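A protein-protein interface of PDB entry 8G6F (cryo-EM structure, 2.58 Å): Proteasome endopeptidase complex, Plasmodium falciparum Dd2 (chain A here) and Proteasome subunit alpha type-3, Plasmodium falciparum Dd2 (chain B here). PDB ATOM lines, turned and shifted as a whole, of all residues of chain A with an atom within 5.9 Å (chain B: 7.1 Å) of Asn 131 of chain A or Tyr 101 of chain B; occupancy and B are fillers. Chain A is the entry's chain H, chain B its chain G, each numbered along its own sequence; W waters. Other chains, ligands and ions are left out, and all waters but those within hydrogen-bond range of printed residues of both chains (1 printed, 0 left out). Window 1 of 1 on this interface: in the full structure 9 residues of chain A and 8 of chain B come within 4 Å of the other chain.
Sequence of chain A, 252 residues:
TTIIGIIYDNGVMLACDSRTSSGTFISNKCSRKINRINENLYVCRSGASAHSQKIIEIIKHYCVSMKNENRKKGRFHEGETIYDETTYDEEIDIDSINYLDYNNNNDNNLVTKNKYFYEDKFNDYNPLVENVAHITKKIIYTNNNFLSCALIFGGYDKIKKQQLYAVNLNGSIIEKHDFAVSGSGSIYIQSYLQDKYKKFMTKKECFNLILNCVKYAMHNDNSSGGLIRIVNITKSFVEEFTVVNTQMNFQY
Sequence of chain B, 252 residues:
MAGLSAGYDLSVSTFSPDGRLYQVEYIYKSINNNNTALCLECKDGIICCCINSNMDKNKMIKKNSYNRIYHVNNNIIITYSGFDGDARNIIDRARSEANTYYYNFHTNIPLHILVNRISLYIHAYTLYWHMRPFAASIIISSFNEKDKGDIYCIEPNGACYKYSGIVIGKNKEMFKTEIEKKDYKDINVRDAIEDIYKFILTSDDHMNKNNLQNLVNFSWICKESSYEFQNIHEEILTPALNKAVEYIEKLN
Asn 131 of chain A touches just these residues of chain B: Tyr 101 (3.98 Å), Phe 105 (3.1 Å) and Thr 107 (2.8 Å). Of the printed residues of chain A, Ile 113 of chain B touches Asn 70 (3.7 Å). Of the printed residues of chain B, Glu 130 of chain A touches His 106 and Thr 107. Of the printed residues of chain B, His 134 of chain A touches Asn 104, Phe 105 and His 106. Of the printed residues of chain A, His 106 of chain B touches Glu 130 (3.7 Å) and His 134 (3.4 Å). The nearest printed residue of chain A that does not touch Phe 105 of chain B is Ile 135 of chain A (4.02 Å).
Printed residues of chain B that touch a printed residue of chain A: Tyr 101, Asn 104, Phe 105, His 106, Thr 107 and Ile 113. Hydrophobic or aromatic side chains of chain B that line the printed part of chain A: Tyr 101, Phe 105, His 106 and Ile 113. Along chain B the printed residues that touch a printed residue of chain A span positions 101 to 113. Hydrophobic or aromatic side chains of chain A within 4 Å of the printed part of chain B: Met 66, His 134 and Ile 135. Along chain A the printed residues that touch a printed residue of chain B span positions 66 to 135. Among the printed residues, no Asp or Glu carboxylate lies within 4 Å of a Lys or Arg side-chain nitrogen of the other chain.
Met 66 of chain A touches Phe 105 of chain B. Asn 70 of chain A touches Ile 113 of chain B (OD1 to CD1, 3.7 Å). Glu 130 of chain A touches His 106 of chain B (OE2 to ND1, 3.7 Å). OE1 of Glu 130 of chain A touches CG2 of Thr 107 of chain B (3.8 Å). Tyr 101 of chain B touches Asn 131 of chain A (OH to ND2, 3.98 Å). O of Asn 104 of chain B touches C of His 134 of chain A (3.7 Å). CB of His 134 of chain A touches O of Phe 105 of chain B, at 3.97 Å. NE2 of His 134 of chain A touches CG of His 106 of chain B, 3.4 Å away.
Water W1 lies within hydrogen-bond range of the side-chain amide nitrogen of Asn 131 of chain A (2.9 Å) and the side-chain hydroxyl of Tyr 101 of chain B (3.0 Å).
O of Thr 100 of chain B lies within hydrogen-bond range of ND2 of Asn 104 of chain B, at 3.4 Å. The backbone carbonyl oxygen of Met 66 of chain A sits close to the side-chain amide nitrogen of Asn 70 of chain A, at 3.4 Å. ND1 of His 134 of chain A lies close to O of Glu 130 of chain A (3.3 Å).
O of Asn 104 of chain B lies within hydrogen-bond range of N of Ile 135 of chain A, 3.4 Å away. The backbone carbonyl oxygen (O) of Phe 105 of chain B sits close to the side-chain amide oxygen (OD1) of Asn 131 of chain A, 3.1 Å away. OG1 of Thr 107 of chain B sits at hydrogen-bond distance from OD1 of Asn 131 of chain A (2.8 Å).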
ATOM      1  N   MET A  66      27.590   5.431  -8.120  1.00  0.00           N
ATOM      2  CA  MET A  66      27.142   6.740  -7.657  1.00  0.00           C
ATOM      3  C   MET A  66      27.603   7.011  -6.232  1.00  0.00           C
ATOM      4  O   MET A  66      28.054   8.117  -5.919  1.00  0.00           O
ATOM      5  CB  MET A  66      25.621   6.827  -7.745  1.00  0.00           C
ATOM      6  CG  MET A  66      25.087   6.908  -9.158  1.00  0.00           C
ATOM      7  SD  MET A  66      23.518   6.042  -9.371  1.00  0.00           S
ATOM      8  CE  MET A  66      22.397   7.156  -8.543  1.00  0.00           C
ATOM      9  N   ASN A  70      30.057   9.985  -4.941  1.00  0.00           N
ATOM     10  CA  ASN A  70      29.485  10.982  -4.043  1.00  0.00           C
ATOM     11  C   ASN A  70      30.408  11.353  -2.892  1.00  0.00           C
ATOM     12  O   ASN A  70      30.151  12.357  -2.222  1.00  0.00           O
ATOM     13  CB  ASN A  70      28.170  10.470  -3.462  1.00  0.00           C
ATOM     14  CG  ASN A  70      26.968  10.898  -4.264  1.00  0.00           C
ATOM     15  OD1 ASN A  70      26.999  11.898  -4.977  1.00  0.00           O
ATOM     16  ND2 ASN A  70      25.891  10.136  -4.148  1.00  0.00           N
ATOM     17  N   PRO A 127      23.481   7.631  -2.125  1.00  0.00           N
ATOM     18  CA  PRO A 127      22.757   8.216  -3.255  1.00  0.00           C
ATOM     19  C   PRO A 127      21.320   8.550  -2.891  1.00  0.00           C
ATOM     20  O   PRO A 127      20.764   8.068  -1.904  1.00  0.00           O
ATOM     21  CB  PRO A 127      22.819   7.123  -4.325  1.00  0.00           C
ATOM     22  CG  PRO A 127      23.976   6.304  -3.953  1.00  0.00           C
ATOM     23  CD  PRO A 127      24.010   6.302  -2.466  1.00  0.00           C
ATOM     24  N   LEU A 128      20.720   9.399  -3.716  1.00  0.00           N
ATOM     25  CA  LEU A 128      19.363   9.861  -3.481  1.00  0.00           C
ATOM     26  C   LEU A 128      18.343   8.905  -4.084  1.00  0.00           C
ATOM     27  O   LEU A 128      18.568   8.284  -5.132  1.00  0.00           O
ATOM     28  CB  LEU A 128      19.164  11.263  -4.056  1.00  0.00           C
ATOM     29  CG  LEU A 128      20.041  12.362  -3.455  1.00  0.00           C
ATOM     30  CD1 LEU A 128      19.910  13.640  -4.253  1.00  0.00           C
ATOM     31  CD2 LEU A 128      19.678  12.604  -2.006  1.00  0.00           C
ATOM     32  N   VAL A 129      17.204   8.800  -3.400  1.00  0.00           N
ATOM     33  CA  VAL A 129      16.135   7.917  -3.850  1.00  0.00           C
ATOM     34  C   VAL A 129      15.662   8.332  -5.233  1.00  0.00           C
ATOM     35  O   VAL A 129      15.434   7.488  -6.105  1.00  0.00           O
ATOM     36  CB  VAL A 129      14.981   7.918  -2.831  1.00  0.00           C
ATOM     37  CG1 VAL A 129      13.923   6.902  -3.215  1.00  0.00           C
ATOM     38  CG2 VAL A 129      15.504   7.640  -1.439  1.00  0.00           C
ATOM     39  N   GLU A 130      15.507   9.637  -5.451  1.00  0.00           N
ATOM     40  CA  GLU A 130      15.082  10.124  -6.755  1.00  0.00           C
ATOM     41  C   GLU A 130      16.109   9.795  -7.829  1.00  0.00           C
ATOM     42  O   GLU A 130      15.745   9.424  -8.948  1.00  0.00           O
ATOM     43  CB  GLU A 130      14.835  11.628  -6.691  1.00  0.00           C
ATOM     44  CG  GLU A 130      14.227  12.207  -7.950  1.00  0.00           C
ATOM     45  CD  GLU A 130      13.924  13.680  -7.817  1.00  0.00           C
ATOM     46  OE1 GLU A 130      14.720  14.390  -7.168  1.00  0.00           O
ATOM     47  OE2 GLU A 130      12.891  14.129  -8.354  1.00  0.00           O
ATOM     48  N   ASN A 131      17.398   9.928  -7.513  1.00  0.00           N
ATOM     49  CA  ASN A 131      18.437   9.612  -8.488  1.00  0.00           C
ATOM     50  C   ASN A 131      18.364   8.153  -8.915  1.00  0.00           C
ATOM     51  O   ASN A 131      18.389   7.839 -10.114  1.00  0.00           O
ATOM     52  CB  ASN A 131      19.814   9.920  -7.904  1.00  0.00           C
ATOM     53  CG  ASN A 131      20.040  11.396  -7.699  1.00  0.00           C
ATOM     54  OD1 ASN A 131      19.162  12.212  -7.964  1.00  0.00           O
ATOM     55  ND2 ASN A 131      21.222  11.749  -7.224  1.00  0.00           N
ATOM     56  N   VAL A 132      18.279   7.243  -7.945  1.00  0.00           N
ATOM     57  CA  VAL A 132      18.234   5.825  -8.286  1.00  0.00           C
ATOM     58  C   VAL A 132      16.952   5.496  -9.046  1.00  0.00           C
ATOM     59  O   VAL A 132      16.972   4.770 -10.050  1.00  0.00           O
ATOM     60  CB  VAL A 132      18.386   4.972  -7.017  1.00  0.00           C
ATOM     61  CG1 VAL A 132      18.263   3.502  -7.343  1.00  0.00           C
ATOM     62  CG2 VAL A 132      19.718   5.259  -6.357  1.00  0.00           C
ATOM     63  N   ALA A 133      15.820   6.038  -8.595  1.00  0.00           N
ATOM     64  CA  ALA A 133      14.559   5.772  -9.272  1.00  0.00           C
ATOM     65  C   ALA A 133      14.587   6.275 -10.706  1.00  0.00           C
ATOM     66  O   ALA A 133      14.075   5.613 -11.612  1.00  0.00           O
ATOM     67  CB  ALA A 133      13.410   6.413  -8.500  1.00  0.00           C
ATOM     68  N   HIS A 134      15.192   7.438 -10.940  1.00  0.00           N
ATOM     69  CA  HIS A 134      15.183   8.013 -12.277  1.00  0.00           C
ATOM     70  C   HIS A 134      16.155   7.307 -13.208  1.00  0.00           C
ATOM     71  O   HIS A 134      15.864   7.154 -14.398  1.00  0.00           O
ATOM     72  CB  HIS A 134      15.492   9.505 -12.209  1.00  0.00           C
ATOM     73  CG  HIS A 134      14.266  10.360 -12.234  1.00  0.00           C
ATOM     74  ND1 HIS A 134      13.601  10.738 -11.090  1.00  0.00           N
ATOM     75  CD2 HIS A 134      13.564  10.879 -13.268  1.00  0.00           C
ATOM     76  CE1 HIS A 134      12.551  11.469 -11.415  1.00  0.00           C
ATOM     77  NE2 HIS A 134      12.506  11.570 -12.731  1.00  0.00           N
ATOM     78  N   ILE A 135      17.305   6.856 -12.708  1.00  0.00           N
ATOM     79  CA  ILE A 135      18.169   6.059 -13.572  1.00  0.00           C
ATOM     80  C   ILE A 135      17.477   4.748 -13.933  1.00  0.00           C
ATOM     81  O   ILE A 135      17.547   4.285 -15.080  1.00  0.00           O
ATOM     82  CB  ILE A 135      19.552   5.840 -12.923  1.00  0.00           C
ATOM     83  CG1 ILE A 135      20.542   5.267 -13.937  1.00  0.00           C
ATOM     84  CG2 ILE A 135      19.473   4.932 -11.719  1.00  0.00           C
ATOM     85  CD1 ILE A 135      20.758   6.126 -15.150  1.00  0.00           C
ATOM     86  N   THR A 136      16.766   4.145 -12.975  1.00  0.00           N
ATOM     87  CA  THR A 136      15.989   2.949 -13.290  1.00  0.00           C
ATOM     88  C   THR A 136      14.931   3.239 -14.344  1.00  0.00           C
ATOM     89  O   THR A 136      14.734   2.450 -15.275  1.00  0.00           O
ATOM     90  CB  THR A 136      15.332   2.405 -12.025  1.00  0.00           C
ATOM     91  OG1 THR A 136      16.325   2.213 -11.012  1.00  0.00           O
ATOM     92  CG2 THR A 136      14.634   1.092 -12.307  1.00  0.00           C
ATOM     93  N   ARG B  95      29.286  21.835 -19.480  1.00  0.00           N
ATOM     94  CA  ARG B  95      27.852  21.877 -19.735  1.00  0.00           C
ATOM     95  C   ARG B  95      27.337  20.521 -20.197  1.00  0.00           C
ATOM     96  O   ARG B  95      26.240  20.101 -19.813  1.00  0.00           O
ATOM     97  CB  ARG B  95      27.543  22.954 -20.769  1.00  0.00           C
ATOM     98  CG  ARG B  95      27.448  24.330 -20.171  1.00  0.00           C
ATOM     99  CD  ARG B  95      27.849  25.395 -21.153  1.00  0.00           C
ATOM    100  NE  ARG B  95      27.807  26.719 -20.548  1.00  0.00           N
ATOM    101  CZ  ARG B  95      28.062  27.845 -21.196  1.00  0.00           C
ATOM    102  NH1 ARG B  95      28.391  27.846 -22.475  1.00  0.00           N
ATOM    103  NH2 ARG B  95      27.977  29.000 -20.545  1.00  0.00           N
ATOM    104  N   SER B  96      28.113  19.821 -21.022  1.00  0.00           N
ATOM    105  CA  SER B  96      27.712  18.494 -21.474  1.00  0.00           C
ATOM    106  C   SER B  96      27.608  17.523 -20.305  1.00  0.00           C
ATOM    107  O   SER B  96      26.667  16.723 -20.230  1.00  0.00           O
ATOM    108  CB  SER B  96      28.713  17.986 -22.509  1.00  0.00           C
ATOM    109  OG  SER B  96      28.172  16.934 -23.280  1.00  0.00           O
ATOM    110  N   GLU B  97      28.572  17.570 -19.385  1.00  0.00           N
ATOM    111  CA  GLU B  97      28.527  16.698 -18.217  1.00  0.00           C
ATOM    112  C   GLU B  97      27.330  17.022 -17.337  1.00  0.00           C
ATOM    113  O   GLU B  97      26.671  16.116 -16.817  1.00  0.00           O
ATOM    114  CB  GLU B  97      29.822  16.820 -17.417  1.00  0.00           C
ATOM    115  CG  GLU B  97      31.063  16.422 -18.182  1.00  0.00           C
ATOM    116  CD  GLU B  97      31.348  14.943 -18.098  1.00  0.00           C
ATOM    117  OE1 GLU B  97      30.432  14.179 -17.734  1.00  0.00           O
ATOM    118  OE2 GLU B  97      32.489  14.540 -18.404  1.00  0.00           O
ATOM    119  N   ALA B  98      27.038  18.309 -17.149  1.00  0.00           N
ATOM    120  CA  ALA B  98      25.857  18.682 -16.377  1.00  0.00           C
ATOM    121  C   ALA B  98      24.586  18.159 -17.034  1.00  0.00           C
ATOM    122  O   ALA B  98      23.689  17.641 -16.354  1.00  0.00           O
ATOM    123  CB  ALA B  98      25.795  20.198 -16.218  1.00  0.00           C
ATOM    124  N   ASN B  99      24.492  18.278 -18.359  1.00  0.00           N
ATOM    125  CA  ASN B  99      23.310  17.787 -19.055  1.00  0.00           C
ATOM    126  C   ASN B  99      23.166  16.283 -18.904  1.00  0.00           C
ATOM    127  O   ASN B  99      22.063  15.779 -18.667  1.00  0.00           O
ATOM    128  CB  ASN B  99      23.372  18.158 -20.535  1.00  0.00           C
ATOM    129  CG  ASN B  99      23.221  19.636 -20.771  1.00  0.00           C
ATOM    130  OD1 ASN B  99      22.801  20.378 -19.889  1.00  0.00           O
ATOM    131  ND2 ASN B  99      23.560  20.075 -21.972  1.00  0.00           N
ATOM    132  N   THR B 100      24.265  15.544 -19.056  1.00  0.00           N
ATOM    133  CA  THR B 100      24.198  14.097 -18.910  1.00  0.00           C
ATOM    134  C   THR B 100      23.799  13.707 -17.497  1.00  0.00           C
ATOM    135  O   THR B 100      23.009  12.777 -17.301  1.00  0.00           O
ATOM    136  CB  THR B 100      25.536  13.465 -19.278  1.00  0.00           C
ATOM    137  OG1 THR B 100      25.879  13.816 -20.622  1.00  0.00           O
ATOM    138  CG2 THR B 100      25.457  11.959 -19.168  1.00  0.00           C
ATOM    139  N   TYR B 101      24.341  14.398 -16.493  1.00  0.00           N
ATOM    140  CA  TYR B 101      23.987  14.078 -15.117  1.00  0.00           C
ATOM    141  C   TYR B 101      22.507  14.310 -14.868  1.00  0.00           C
ATOM    142  O   TYR B 101      21.844  13.493 -14.219  1.00  0.00           O
ATOM    143  CB  TYR B 101      24.825  14.907 -14.149  1.00  0.00           C
ATOM    144  CG  TYR B 101      24.773  14.402 -12.730  1.00  0.00           C
ATOM    145  CD1 TYR B 101      23.737  14.759 -11.884  1.00  0.00           C
ATOM    146  CD2 TYR B 101      25.756  13.561 -12.238  1.00  0.00           C
ATOM    147  CE1 TYR B 101      23.684  14.296 -10.593  1.00  0.00           C
ATOM    148  CE2 TYR B 101      25.712  13.098 -10.951  1.00  0.00           C
ATOM    149  CZ  TYR B 101      24.676  13.468 -10.132  1.00  0.00           C
ATOM    150  OH  TYR B 101      24.632  13.003  -8.844  1.00  0.00           O
ATOM    151  N   TYR B 102      21.966  15.420 -15.370  1.00  0.00           N
ATOM    152  CA  TYR B 102      20.539  15.660 -15.193  1.00  0.00           C
ATOM    153  C   TYR B 102      19.705  14.621 -15.936  1.00  0.00           C
ATOM    154  O   TYR B 102      18.686  14.156 -15.418  1.00  0.00           O
ATOM    155  CB  TYR B 102      20.168  17.065 -15.650  1.00  0.00           C
ATOM    156  CG  TYR B 102      18.729  17.398 -15.351  1.00  0.00           C
ATOM    157  CD1 TYR B 102      17.726  17.113 -16.265  1.00  0.00           C
ATOM    158  CD2 TYR B 102      18.368  17.972 -14.143  1.00  0.00           C
ATOM    159  CE1 TYR B 102      16.413  17.402 -15.988  1.00  0.00           C
ATOM    160  CE2 TYR B 102      17.060  18.262 -13.859  1.00  0.00           C
ATOM    161  CZ  TYR B 102      16.085  17.976 -14.785  1.00  0.00           C
ATOM    162  OH  TYR B 102      14.772  18.269 -14.505  1.00  0.00           O
ATOM    163  N   TYR B 103      20.114  14.251 -17.151  1.00  0.00           N
ATOM    164  CA  TYR B 103      19.384  13.229 -17.893  1.00  0.00           C
ATOM    165  C   TYR B 103      19.370  11.914 -17.132  1.00  0.00           C
ATOM    166  O   TYR B 103      18.358  11.207 -17.114  1.00  0.00           O
ATOM    167  CB  TYR B 103      20.012  13.016 -19.270  1.00  0.00           C
ATOM    168  CG  TYR B 103      19.540  13.951 -20.355  1.00  0.00           C
ATOM    169  CD1 TYR B 103      18.190  14.190 -20.565  1.00  0.00           C
ATOM    170  CD2 TYR B 103      20.451  14.587 -21.188  1.00  0.00           C
ATOM    171  CE1 TYR B 103      17.766  15.042 -21.562  1.00  0.00           C
ATOM    172  CE2 TYR B 103      20.037  15.436 -22.184  1.00  0.00           C
ATOM    173  CZ  TYR B 103      18.694  15.661 -22.370  1.00  0.00           C
ATOM    174  OH  TYR B 103      18.283  16.513 -23.368  1.00  0.00           O
ATOM    175  N   ASN B 104      20.495  11.559 -16.514  1.00  0.00           N
ATOM    176  CA  ASN B 104      20.594  10.280 -15.824  1.00  0.00           C
ATOM    177  C   ASN B 104      19.801  10.281 -14.526  1.00  0.00           C
ATOM    178  O   ASN B 104      19.065   9.332 -14.240  1.00  0.00           O
ATOM    179  CB  ASN B 104      22.058   9.953 -15.547  1.00  0.00           C
ATOM    180  CG  ASN B 104      22.751   9.341 -16.735  1.00  0.00           C
ATOM    181  OD1 ASN B 104      22.127   8.676 -17.556  1.00  0.00           O
ATOM    182  ND2 ASN B 104      24.051   9.564 -16.836  1.00  0.00           N
ATOM    183  N   PHE B 105      19.930  11.339 -13.728  1.00  0.00           N
ATOM    184  CA  PHE B 105      19.484  11.302 -12.344  1.00  0.00           C
ATOM    185  C   PHE B 105      18.444  12.349 -11.987  1.00  0.00           C
ATOM    186  O   PHE B 105      17.941  12.327 -10.859  1.00  0.00           O
ATOM    187  CB  PHE B 105      20.692  11.450 -11.409  1.00  0.00           C
ATOM    188  CG  PHE B 105      21.802  10.495 -11.719  1.00  0.00           C
ATOM    189  CD1 PHE B 105      21.600   9.133 -11.626  1.00  0.00           C
ATOM    190  CD2 PHE B 105      23.035  10.952 -12.127  1.00  0.00           C
ATOM    191  CE1 PHE B 105      22.607   8.252 -11.922  1.00  0.00           C
ATOM    192  CE2 PHE B 105      24.045  10.075 -12.421  1.00  0.00           C
ATOM    193  CZ  PHE B 105      23.831   8.724 -12.319  1.00  0.00           C
ATOM    194  N   HIS B 106      18.099  13.254 -12.897  1.00  0.00           N
ATOM    195  CA  HIS B 106      17.037  14.228 -12.683  1.00  0.00           C
ATOM    196  C   HIS B 106      17.362  15.226 -11.581  1.00  0.00           C
ATOM    197  O   HIS B 106      16.458  15.842 -11.017  1.00  0.00           O
ATOM    198  CB  HIS B 106      15.714  13.528 -12.368  1.00  0.00           C
ATOM    199  CG  HIS B 106      14.506  14.317 -12.758  1.00  0.00           C
ATOM    200  ND1 HIS B 106      13.703  14.948 -11.835  1.00  0.00           N
ATOM    201  CD2 HIS B 106      13.966  14.578 -13.970  1.00  0.00           C
ATOM    202  CE1 HIS B 106      12.719  15.565 -12.463  1.00  0.00           C
ATOM    203  NE2 HIS B 106      12.855  15.356 -13.759  1.00  0.00           N
ATOM    204  N   THR B 107      18.637  15.395 -11.251  1.00  0.00           N
ATOM    205  CA  THR B 107      19.076  16.436 -10.337  1.00  0.00           C
ATOM    206  C   THR B 107      20.295  17.107 -10.941  1.00  0.00           C
ATOM    207  O   THR B 107      20.906  16.599 -11.882  1.00  0.00           O
ATOM    208  CB  THR B 107      19.400  15.887  -8.941  1.00  0.00           C
ATOM    209  OG1 THR B 107      20.111  14.651  -9.058  1.00  0.00           O
ATOM    210  CG2 THR B 107      18.131  15.661  -8.144  1.00  0.00           C
ATOM    211  N   ASN B 108      20.641  18.270 -10.401  1.00  0.00           N
ATOM    212  CA  ASN B 108      21.817  18.988 -10.867  1.00  0.00           C
ATOM    213  C   ASN B 108      23.089  18.302 -10.388  1.00  0.00           C
ATOM    214  O   ASN B 108      23.144  17.768  -9.278  1.00  0.00           O
ATOM    215  CB  ASN B 108      21.785  20.428 -10.370  1.00  0.00           C
ATOM    216  CG  ASN B 108      20.835  21.291 -11.156  1.00  0.00           C
ATOM    217  OD1 ASN B 108      20.402  20.926 -12.246  1.00  0.00           O
ATOM    218  ND2 ASN B 108      20.506  22.449 -10.608  1.00  0.00           N
ATOM    219  N   ILE B 109      24.116  18.329 -11.228  1.00  0.00           N
ATOM    220  CA  ILE B 109      25.379  17.661 -10.892  1.00  0.00           C
ATOM    221  C   ILE B 109      26.016  18.360  -9.695  1.00  0.00           C
ATOM    222  O   ILE B 109      26.077  19.601  -9.670  1.00  0.00           O
ATOM    223  CB  ILE B 109      26.322  17.665 -12.100  1.00  0.00           C
ATOM    224  CG1 ILE B 109      27.536  16.775 -11.829  1.00  0.00           C
ATOM    225  CG2 ILE B 109      26.774  19.076 -12.432  1.00  0.00           C
ATOM    226  CD1 ILE B 109      28.297  16.395 -13.064  1.00  0.00           C
ATOM    227  N   PRO B 110      26.481  17.629  -8.683  1.00  0.00           N
ATOM    228  CA  PRO B 110      27.217  18.276  -7.593  1.00  0.00           C
ATOM    229  C   PRO B 110      28.514  18.909  -8.077  1.00  0.00           C
ATOM    230  O   PRO B 110      29.148  18.447  -9.031  1.00  0.00           O
ATOM    231  CB  PRO B 110      27.483  17.130  -6.615  1.00  0.00           C
ATOM    232  CG  PRO B 110      26.421  16.146  -6.896  1.00  0.00           C
ATOM    233  CD  PRO B 110      26.152  16.232  -8.360  1.00  0.00           C
ATOM    234  N   ILE B 113      31.659  16.646  -8.056  1.00  0.00           N
ATOM    235  CA  ILE B 113      31.625  15.668  -9.140  1.00  0.00           C
ATOM    236  C   ILE B 113      31.969  16.334 -10.463  1.00  0.00           C
ATOM    237  O   ILE B 113      32.747  15.798 -11.263  1.00  0.00           O
ATOM    238  CB  ILE B 113      30.251  14.974  -9.197  1.00  0.00           C
ATOM    239  CG1 ILE B 113      30.032  14.152  -7.927  1.00  0.00           C
ATOM    240  CG2 ILE B 113      30.151  14.092 -10.439  1.00  0.00           C
ATOM    241  CD1 ILE B 113      28.784  13.324  -7.930  1.00  0.00           C
ATOM    242  N   LEU B 114      31.393  17.509 -10.721  1.00  0.00           N
ATOM    243  CA  LEU B 114      31.702  18.207 -11.962  1.00  0.00           C
ATOM    244  C   LEU B 114      33.177  18.580 -12.024  1.00  0.00           C
ATOM    245  O   LEU B 114      33.812  18.470 -13.078  1.00  0.00           O
ATOM    246  CB  LEU B 114      30.828  19.451 -12.100  1.00  0.00           C
ATOM    247  CG  LEU B 114      30.995  20.240 -13.400  1.00  0.00           C
ATOM    248  CD1 LEU B 114      30.488  19.447 -14.585  1.00  0.00           C
ATOM    249  CD2 LEU B 114      30.284  21.571 -13.306  1.00  0.00           C
ATOM    250  N   ARG B 117      35.195  15.477 -12.888  1.00  0.00           N
ATOM    251  CA  ARG B 117      35.045  15.079 -14.283  1.00  0.00           C
ATOM    252  C   ARG B 117      35.791  16.028 -15.214  1.00  0.00           C
ATOM    253  O   ARG B 117      36.406  15.591 -16.192  1.00  0.00           O
ATOM    254  CB  ARG B 117      33.564  15.006 -14.644  1.00  0.00           C
ATOM    255  CG  ARG B 117      32.915  13.725 -14.167  1.00  0.00           C
ATOM    256  CD  ARG B 117      31.457  13.665 -14.523  1.00  0.00           C
ATOM    257  NE  ARG B 117      30.763  12.621 -13.782  1.00  0.00           N
ATOM    258  CZ  ARG B 117      29.504  12.266 -13.993  1.00  0.00           C
ATOM    259  NH1 ARG B 117      28.769  12.846 -14.926  1.00  0.00           N
ATOM    260  NH2 ARG B 117      28.970  11.305 -13.249  1.00  0.00           N
HETATM  261  O   HOH W   1      22.880  14.131  -6.733  1.00  0.00           O
